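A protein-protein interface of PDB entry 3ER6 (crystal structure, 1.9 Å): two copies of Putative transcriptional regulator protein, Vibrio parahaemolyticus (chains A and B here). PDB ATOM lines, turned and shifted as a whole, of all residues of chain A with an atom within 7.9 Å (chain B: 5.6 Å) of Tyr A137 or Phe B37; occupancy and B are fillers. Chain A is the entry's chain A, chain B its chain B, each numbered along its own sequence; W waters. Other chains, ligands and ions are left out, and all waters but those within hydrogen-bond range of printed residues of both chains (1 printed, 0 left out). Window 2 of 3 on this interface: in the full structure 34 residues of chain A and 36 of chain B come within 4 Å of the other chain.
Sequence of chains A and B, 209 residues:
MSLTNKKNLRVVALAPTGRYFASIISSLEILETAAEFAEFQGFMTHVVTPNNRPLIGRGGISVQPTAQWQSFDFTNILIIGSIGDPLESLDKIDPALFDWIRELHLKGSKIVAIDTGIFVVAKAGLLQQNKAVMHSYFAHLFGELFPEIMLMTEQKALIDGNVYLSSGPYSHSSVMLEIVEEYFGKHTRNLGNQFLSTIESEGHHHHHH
OG1 of Thr B33 is in hydrogen-bond range of OH of Tyr A20, 2.6 Å away. The backbone NH (N) of Tyr A137 is in hydrogen-bond range of the side-chain hydroxyl (OG1) of Thr B198 (2.9 Å).
The side-chain carboxylate (OD1) of Asp A115 sits at hydrogen-bond distance from a ring nitrogen (NE2) of His A135 (2.8 Å). SD of Met A134 sits at hydrogen-bond distance from NE2 of His A135 (3.8 Å). The backbone carbonyl oxygen (O) of Gln B194 is in hydrogen-bond range of the side-chain hydroxyl (OG1) of Thr B198.
His A135 touches Thr B198 (CG to CG2, 3.6 Å). N of Ser A136 touches OG1 of Thr B198, at 3.6 Å. CE1 of Phe B37 touches OH of Tyr A137, at 3.2 Å. Gln B194 touches Tyr A137 (C to CD1, 3.9 Å). Tyr A137 touches Phe B195. Thr B198 touches Pro A169.
Phe B37 touches just one residue of chain A: Tyr A137 (3.2 Å). Printed residues of chain A within 4 Å of Gln B194: Tyr A137. Of the printed residues of chain A, Thr B33 touches Tyr A20 (2.6 Å). The nearest residue of chain A that does not touch Phe B37 is Tyr A20 (7.0 Å).
Of the 17 printed residues of chain A, 5 touch a printed residue of chain B. Printed residues of chain A that touch a printed residue of chain B: Tyr A20, His A135, Ser A136, Tyr A137 and Pro A169. Hydrophobic or aromatic side chains of chain A within 4 Å of the printed part of chain B: Tyr A20, His A135, Tyr A137 and Pro A169. Hydrophobic or aromatic side chains of chain B within 4 Å of the printed part of chain A: Phe B37 and Phe B195. Among the printed residues, 8 pairs touch across the chains. Among the printed residues, no Asp or Glu carboxylate lies within 4 Å of a Lys or Arg side-chain nitrogen of the other chain.
No position is printed for both chains.
Water W1 bridges the side-chain carboxylate of Glu B36 and the side-chain hydroxyl of Tyr A20.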
ATOM      1  N   TYR A  20      24.310 -11.146   9.728  1.00  0.00           N
ATOM      2  CA  TYR A  20      24.807 -12.457  10.082  1.00  0.00           C
ATOM      3  C   TYR A  20      24.259 -13.444   9.086  1.00  0.00           C
ATOM      4  O   TYR A  20      23.292 -14.160   9.375  1.00  0.00           O
ATOM      5  CB  TYR A  20      24.329 -12.832  11.518  1.00  0.00           C
ATOM      6  CG  TYR A  20      24.996 -11.933  12.544  1.00  0.00           C
ATOM      7  CD1 TYR A  20      26.360 -12.073  12.832  1.00  0.00           C
ATOM      8  CD2 TYR A  20      24.278 -10.914  13.197  1.00  0.00           C
ATOM      9  CE1 TYR A  20      26.989 -11.219  13.801  1.00  0.00           C
ATOM     10  CE2 TYR A  20      24.887 -10.044  14.099  1.00  0.00           C
ATOM     11  CZ  TYR A  20      26.210 -10.197  14.416  1.00  0.00           C
ATOM     12  OH  TYR A  20      26.782  -9.340  15.346  1.00  0.00           O
ATOM     13  N   GLY A  84      20.372 -12.518  14.221  1.00  0.00           N
ATOM     14  CA  GLY A  84      21.134 -11.546  15.041  1.00  0.00           C
ATOM     15  C   GLY A  84      20.601 -11.525  16.480  1.00  0.00           C
ATOM     16  O   GLY A  84      20.311 -12.561  17.041  1.00  0.00           O
ATOM     17  N   ASP A  85      20.425 -10.348  17.045  1.00  0.00           N
ATOM     18  CA  ASP A  85      19.937 -10.246  18.397  1.00  0.00           C
ATOM     19  C   ASP A  85      18.441 -10.428  18.410  1.00  0.00           C
ATOM     20  O   ASP A  85      17.686  -9.577  17.903  1.00  0.00           O
ATOM     21  CB  ASP A  85      20.297  -8.883  18.983  1.00  0.00           C
ATOM     22  CG  ASP A  85      19.812  -8.708  20.432  1.00  0.00           C
ATOM     23  OD1 ASP A  85      19.119  -9.567  21.044  1.00  0.00           O
ATOM     24  OD2 ASP A  85      20.141  -7.640  20.965  1.00  0.00           O
ATOM     25  N   PRO A  86      17.998 -11.532  19.017  1.00  0.00           N
ATOM     26  CA  PRO A  86      16.559 -11.873  18.977  1.00  0.00           C
ATOM     27  C   PRO A  86      15.705 -10.786  19.616  1.00  0.00           C
ATOM     28  O   PRO A  86      14.531 -10.619  19.263  1.00  0.00           O
ATOM     29  CB  PRO A  86      16.471 -13.199  19.730  1.00  0.00           C
ATOM     30  CG  PRO A  86      17.902 -13.799  19.603  1.00  0.00           C
ATOM     31  CD  PRO A  86      18.829 -12.575  19.639  1.00  0.00           C
ATOM     32  N   ASP A 115      22.601 -20.942  14.772  1.00  0.00           N
ATOM     33  CA  ASP A 115      22.819 -19.705  15.457  1.00  0.00           C
ATOM     34  C   ASP A 115      21.439 -19.290  16.012  1.00  0.00           C
ATOM     35  O   ASP A 115      20.641 -20.166  16.391  1.00  0.00           O
ATOM     36  CB  ASP A 115      23.410 -18.635  14.511  1.00  0.00           C
ATOM     37  CG  ASP A 115      23.982 -17.379  15.271  1.00  0.00           C
ATOM     38  OD1 ASP A 115      24.057 -17.331  16.522  1.00  0.00           O
ATOM     39  OD2 ASP A 115      24.378 -16.433  14.592  1.00  0.00           O
ATOM     40  N   THR A 116      21.157 -17.995  16.061  1.00  0.00           N
ATOM     41  CA  THR A 116      19.850 -17.520  16.618  1.00  0.00           C
ATOM     42  C   THR A 116      18.584 -17.921  15.788  1.00  0.00           C
ATOM     43  O   THR A 116      17.461 -17.717  16.225  1.00  0.00           O
ATOM     44  CB  THR A 116      19.851 -16.017  16.951  1.00  0.00           C
ATOM     45  OG1 THR A 116      20.155 -15.240  15.794  1.00  0.00           O
ATOM     46  CG2 THR A 116      20.889 -15.721  18.036  1.00  0.00           C
ATOM     47  N   PHE A 119      16.077 -19.572  17.873  1.00  0.00           N
ATOM     48  CA  PHE A 119      15.017 -18.832  18.544  1.00  0.00           C
ATOM     49  C   PHE A 119      13.741 -18.895  17.673  1.00  0.00           C
ATOM     50  O   PHE A 119      12.619 -18.894  18.214  1.00  0.00           O
ATOM     51  CB  PHE A 119      15.401 -17.352  18.766  1.00  0.00           C
ATOM     52  CG  PHE A 119      16.346 -17.126  19.918  1.00  0.00           C
ATOM     53  CD1 PHE A 119      17.668 -17.589  19.871  1.00  0.00           C
ATOM     54  CD2 PHE A 119      15.913 -16.429  21.062  1.00  0.00           C
ATOM     55  CE1 PHE A 119      18.534 -17.364  20.937  1.00  0.00           C
ATOM     56  CE2 PHE A 119      16.781 -16.228  22.131  1.00  0.00           C
ATOM     57  CZ  PHE A 119      18.089 -16.682  22.058  1.00  0.00           C
ATOM     58  N   MET A 134      22.015 -23.592  22.842  1.00  0.00           N
ATOM     59  CA  MET A 134      22.333 -22.243  22.387  1.00  0.00           C
ATOM     60  C   MET A 134      23.741 -21.957  22.833  1.00  0.00           C
ATOM     61  O   MET A 134      24.181 -22.553  23.845  1.00  0.00           O
ATOM     62  CB  MET A 134      21.336 -21.212  22.942  1.00  0.00           C
ATOM     63  CG  MET A 134      21.585 -19.737  22.536  1.00  0.00           C
ATOM     64  SD  MET A 134      21.855 -19.346  20.736  1.00  0.00           S
ATOM     65  CE  MET A 134      20.460 -20.138  20.055  1.00  0.00           C
ATOM     66  N   HIS A 135      24.466 -21.092  22.117  1.00  0.00           N
ATOM     67  CA  HIS A 135      25.816 -20.764  22.537  1.00  0.00           C
ATOM     68  C   HIS A 135      25.754 -19.786  23.730  1.00  0.00           C
ATOM     69  O   HIS A 135      24.683 -19.207  24.050  1.00  0.00           O
ATOM     70  CB  HIS A 135      26.656 -20.204  21.362  1.00  0.00           C
ATOM     71  CG  HIS A 135      25.968 -19.135  20.579  1.00  0.00           C
ATOM     72  ND1 HIS A 135      25.626 -17.922  21.123  1.00  0.00           N
ATOM     73  CD2 HIS A 135      25.512 -19.117  19.294  1.00  0.00           C
ATOM     74  CE1 HIS A 135      25.011 -17.190  20.206  1.00  0.00           C
ATOM     75  NE2 HIS A 135      24.926 -17.895  19.092  1.00  0.00           N
ATOM     76  N   SER A 136      26.884 -19.588  24.399  1.00  0.00           N
ATOM     77  CA  SER A 136      26.918 -18.795  25.619  1.00  0.00           C
ATOM     78  C   SER A 136      26.505 -17.347  25.429  1.00  0.00           C
ATOM     79  O   SER A 136      25.972 -16.722  26.344  1.00  0.00           O
ATOM     80  CB  SER A 136      28.322 -18.836  26.250  1.00  0.00           C
ATOM     81  OG  SER A 136      28.629 -20.159  26.663  1.00  0.00           O
ATOM     82  N   TYR A 137      26.771 -16.793  24.247  1.00  0.00           N
ATOM     83  CA  TYR A 137      26.456 -15.379  24.066  1.00  0.00           C
ATOM     84  C   TYR A 137      24.928 -15.130  24.201  1.00  0.00           C
ATOM     85  O   TYR A 137      24.500 -14.145  24.832  1.00  0.00           O
ATOM     86  CB  TYR A 137      26.985 -14.835  22.731  1.00  0.00           C
ATOM     87  CG  TYR A 137      26.850 -13.335  22.700  1.00  0.00           C
ATOM     88  CD1 TYR A 137      27.595 -12.552  23.557  1.00  0.00           C
ATOM     89  CD2 TYR A 137      25.927 -12.711  21.878  1.00  0.00           C
ATOM     90  CE1 TYR A 137      27.474 -11.184  23.562  1.00  0.00           C
ATOM     91  CE2 TYR A 137      25.778 -11.350  21.893  1.00  0.00           C
ATOM     92  CZ  TYR A 137      26.557 -10.594  22.737  1.00  0.00           C
ATOM     93  OH  TYR A 137      26.409  -9.243  22.759  1.00  0.00           O
ATOM     94  N   PHE A 138      24.104 -16.013  23.641  1.00  0.00           N
ATOM     95  CA  PHE A 138      22.659 -15.815  23.743  1.00  0.00           C
ATOM     96  C   PHE A 138      21.888 -16.801  24.664  1.00  0.00           C
ATOM     97  O   PHE A 138      20.652 -16.804  24.666  1.00  0.00           O
ATOM     98  CB  PHE A 138      22.005 -15.692  22.345  1.00  0.00           C
ATOM     99  CG  PHE A 138      22.153 -14.300  21.736  1.00  0.00           C
ATOM    100  CD1 PHE A 138      21.722 -13.176  22.441  1.00  0.00           C
ATOM    101  CD2 PHE A 138      22.710 -14.108  20.483  1.00  0.00           C
ATOM    102  CE1 PHE A 138      21.845 -11.910  21.929  1.00  0.00           C
ATOM    103  CE2 PHE A 138      22.851 -12.841  19.974  1.00  0.00           C
ATOM    104  CZ  PHE A 138      22.427 -11.738  20.697  1.00  0.00           C
ATOM    105  N   ALA A 139      22.600 -17.615  25.451  1.00  0.00           N
ATOM    106  CA  ALA A 139      21.913 -18.624  26.263  1.00  0.00           C
ATOM    107  C   ALA A 139      21.010 -18.026  27.348  1.00  0.00           C
ATOM    108  O   ALA A 139      19.901 -18.547  27.626  1.00  0.00           O
ATOM    109  CB  ALA A 139      22.897 -19.620  26.909  1.00  0.00           C
ATOM    110  N   HIS A 140      21.474 -16.939  27.974  1.00  0.00           N
ATOM    111  CA  HIS A 140      20.632 -16.276  28.973  1.00  0.00           C
ATOM    112  C   HIS A 140      19.288 -15.817  28.381  1.00  0.00           C
ATOM    113  O   HIS A 140      18.224 -16.092  28.914  1.00  0.00           O
ATOM    114  CB  HIS A 140      21.347 -15.075  29.597  1.00  0.00           C
ATOM    115  CG  HIS A 140      20.507 -14.380  30.621  1.00  0.00           C
ATOM    116  ND1 HIS A 140      20.302 -14.895  31.888  1.00  0.00           N
ATOM    117  CD2 HIS A 140      19.756 -13.256  30.546  1.00  0.00           C
ATOM    118  CE1 HIS A 140      19.488 -14.096  32.559  1.00  0.00           C
ATOM    119  NE2 HIS A 140      19.141 -13.098  31.765  1.00  0.00           N
ATOM    120  N   LEU A 141      19.354 -15.106  27.261  1.00  0.00           N
ATOM    121  CA  LEU A 141      18.144 -14.611  26.613  1.00  0.00           C
ATOM    122  C   LEU A 141      17.214 -15.758  26.245  1.00  0.00           C
ATOM    123  O   LEU A 141      16.005 -15.686  26.504  1.00  0.00           O
ATOM    124  CB  LEU A 141      18.486 -13.748  25.395  1.00  0.00           C
ATOM    125  CG  LEU A 141      17.298 -13.156  24.616  1.00  0.00           C
ATOM    126  CD1 LEU A 141      16.470 -12.199  25.490  1.00  0.00           C
ATOM    127  CD2 LEU A 141      17.800 -12.396  23.383  1.00  0.00           C
ATOM    128  N   PHE A 142      17.765 -16.812  25.645  1.00  0.00           N
ATOM    129  CA  PHE A 142      16.944 -17.990  25.325  1.00  0.00           C
ATOM    130  C   PHE A 142      16.221 -18.475  26.601  1.00  0.00           C
ATOM    131  O   PHE A 142      15.037 -18.826  26.572  1.00  0.00           O
ATOM    132  CB  PHE A 142      17.795 -19.121  24.801  1.00  0.00           C
ATOM    133  CG  PHE A 142      16.997 -20.211  24.151  1.00  0.00           C
ATOM    134  CD1 PHE A 142      16.722 -20.151  22.794  1.00  0.00           C
ATOM    135  CD2 PHE A 142      16.517 -21.287  24.897  1.00  0.00           C
ATOM    136  CE1 PHE A 142      15.975 -21.146  22.178  1.00  0.00           C
ATOM    137  CE2 PHE A 142      15.779 -22.294  24.291  1.00  0.00           C
ATOM    138  CZ  PHE A 142      15.506 -22.200  22.901  1.00  0.00           C
ATOM    139  N   PRO A 169      28.331 -20.057  16.528  1.00  0.00           N
ATOM    140  CA  PRO A 169      27.671 -19.438  15.346  1.00  0.00           C
ATOM    141  C   PRO A 169      28.222 -19.840  13.957  1.00  0.00           C
ATOM    142  O   PRO A 169      27.467 -19.707  12.961  1.00  0.00           O
ATOM    143  CB  PRO A 169      27.846 -17.921  15.603  1.00  0.00           C
ATOM    144  CG  PRO A 169      29.149 -17.868  16.508  1.00  0.00           C
ATOM    145  CD  PRO A 169      28.960 -19.048  17.412  1.00  0.00           C
ATOM    146  N   THR B  33      31.637  -7.442  14.924  1.00  0.00           N
ATOM    147  CA  THR B  33      30.962  -7.670  16.178  1.00  0.00           C
ATOM    148  C   THR B  33      31.873  -7.409  17.398  1.00  0.00           C
ATOM    149  O   THR B  33      31.481  -6.708  18.332  1.00  0.00           O
ATOM    150  CB  THR B  33      30.313  -9.083  16.254  1.00  0.00           C
ATOM    151  OG1 THR B  33      29.401  -9.244  15.135  1.00  0.00           O
ATOM    152  CG2 THR B  33      29.577  -9.217  17.586  1.00  0.00           C
ATOM    153  N   ALA B  34      33.093  -7.942  17.355  1.00  0.00           N
ATOM    154  CA  ALA B  34      34.098  -7.692  18.406  1.00  0.00           C
ATOM    155  C   ALA B  34      34.265  -6.203  18.684  1.00  0.00           C
ATOM    156  O   ALA B  34      34.316  -5.782  19.849  1.00  0.00           O
ATOM    157  CB  ALA B  34      35.429  -8.296  17.997  1.00  0.00           C
ATOM    158  N   ALA B  35      34.358  -5.420  17.616  1.00  0.00           N
ATOM    159  CA  ALA B  35      34.553  -3.970  17.714  1.00  0.00           C
ATOM    160  C   ALA B  35      33.386  -3.205  18.376  1.00  0.00           C
ATOM    161  O   ALA B  35      33.613  -2.141  18.958  1.00  0.00           O
ATOM    162  CB  ALA B  35      34.847  -3.395  16.367  1.00  0.00           C
ATOM    163  N   GLU B  36      32.160  -3.746  18.283  1.00  0.00           N
ATOM    164  CA  GLU B  36      30.955  -3.203  18.965  1.00  0.00           C
ATOM    165  C   GLU B  36      31.049  -3.311  20.480  1.00  0.00           C
ATOM    166  O   GLU B  36      30.518  -2.484  21.215  1.00  0.00           O
ATOM    167  CB  GLU B  36      29.668  -3.919  18.494  1.00  0.00           C
ATOM    168  CG  GLU B  36      29.366  -3.792  16.981  1.00  0.00           C
ATOM    169  CD  GLU B  36      28.191  -4.683  16.504  1.00  0.00           C
ATOM    170  OE1 GLU B  36      28.015  -4.851  15.261  1.00  0.00           O
ATOM    171  OE2 GLU B  36      27.482  -5.243  17.379  1.00  0.00           O
ATOM    172  N   PHE B  37      31.742  -4.323  20.960  1.00  0.00           N
ATOM    173  CA  PHE B  37      32.072  -4.401  22.365  1.00  0.00           C
ATOM    174  C   PHE B  37      33.167  -3.402  22.781  1.00  0.00           C
ATOM    175  O   PHE B  37      33.376  -3.158  23.969  1.00  0.00           O
ATOM    176  CB  PHE B  37      32.479  -5.839  22.701  1.00  0.00           C
ATOM    177  CG  PHE B  37      31.413  -6.839  22.393  1.00  0.00           C
ATOM    178  CD1 PHE B  37      30.102  -6.633  22.818  1.00  0.00           C
ATOM    179  CD2 PHE B  37      31.705  -7.986  21.689  1.00  0.00           C
ATOM    180  CE1 PHE B  37      29.118  -7.560  22.547  1.00  0.00           C
ATOM    181  CE2 PHE B  37      30.717  -8.919  21.415  1.00  0.00           C
ATOM    182  CZ  PHE B  37      29.428  -8.698  21.838  1.00  0.00           C
ATOM    183  N   ALA B  38      33.894  -2.846  21.814  1.00  0.00           N
ATOM    184  CA  ALA B  38      34.951  -1.883  22.103  1.00  0.00           C
ATOM    185  C   ALA B  38      34.458  -0.456  21.893  1.00  0.00           C
ATOM    186  O   ALA B  38      34.731   0.414  22.727  1.00  0.00           O
ATOM    187  CB  ALA B  38      36.164  -2.134  21.200  1.00  0.00           C
ATOM    188  N   GLN B 194      31.443 -13.026  26.880  1.00  0.00           N
ATOM    189  CA  GLN B 194      30.719 -14.208  26.423  1.00  0.00           C
ATOM    190  C   GLN B 194      30.793 -14.304  24.901  1.00  0.00           C
ATOM    191  O   GLN B 194      30.815 -15.415  24.339  1.00  0.00           O
ATOM    192  CB  GLN B 194      29.272 -14.163  26.893  1.00  0.00           C
ATOM    193  CG  GLN B 194      29.113 -14.721  28.337  1.00  0.00           C
ATOM    194  CD  GLN B 194      28.056 -13.977  29.195  1.00  0.00           C
ATOM    195  OE1 GLN B 194      27.819 -14.341  30.363  1.00  0.00           O
ATOM    196  NE2 GLN B 194      27.428 -12.936  28.625  1.00  0.00           N
ATOM    197  N   PHE B 195      30.866 -13.149  24.243  1.00  0.00           N
ATOM    198  CA  PHE B 195      30.944 -13.183  22.801  1.00  0.00           C
ATOM    199  C   PHE B 195      32.271 -13.829  22.393  1.00  0.00           C
ATOM    200  O   PHE B 195      32.306 -14.741  21.569  1.00  0.00           O
ATOM    201  CB  PHE B 195      30.795 -11.800  22.145  1.00  0.00           C
ATOM    202  CG  PHE B 195      31.130 -11.819  20.676  1.00  0.00           C
ATOM    203  CD1 PHE B 195      30.287 -12.479  19.770  1.00  0.00           C
ATOM    204  CD2 PHE B 195      32.326 -11.266  20.211  1.00  0.00           C
ATOM    205  CE1 PHE B 195      30.607 -12.541  18.415  1.00  0.00           C
ATOM    206  CE2 PHE B 195      32.659 -11.333  18.850  1.00  0.00           C
ATOM    207  CZ  PHE B 195      31.812 -11.963  17.961  1.00  0.00           C
ATOM    208  N   LEU B 196      33.371 -13.356  22.992  1.00  0.00           N
ATOM    209  CA  LEU B 196      34.705 -13.827  22.595  1.00  0.00           C
ATOM    210  C   LEU B 196      34.858 -15.318  22.930  1.00  0.00           C
ATOM    211  O   LEU B 196      35.454 -16.086  22.207  1.00  0.00           O
ATOM    212  CB  LEU B 196      35.830 -12.932  23.168  1.00  0.00           C
ATOM    213  CG  LEU B 196      35.739 -11.544  22.443  1.00  0.00           C
ATOM    214  CD1 LEU B 196      36.737 -10.438  22.926  1.00  0.00           C
ATOM    215  CD2 LEU B 196      35.741 -11.624  20.876  1.00  0.00           C
ATOM    216  N   THR B 198      32.284 -17.399  23.007  1.00  0.00           N
ATOM    217  CA  THR B 198      31.412 -18.113  22.059  1.00  0.00           C
ATOM    218  C   THR B 198      32.174 -18.426  20.759  1.00  0.00           C
ATOM    219  O   THR B 198      32.113 -19.530  20.221  1.00  0.00           O
ATOM    220  CB  THR B 198      30.144 -17.298  21.797  1.00  0.00           C
ATOM    221  OG1 THR B 198      29.301 -17.341  22.950  1.00  0.00           O
ATOM    222  CG2 THR B 198      29.355 -17.868  20.655  1.00  0.00           C
HETATM  223  O   HOH W   1      26.049  -6.175  14.476  1.00  0.00           O
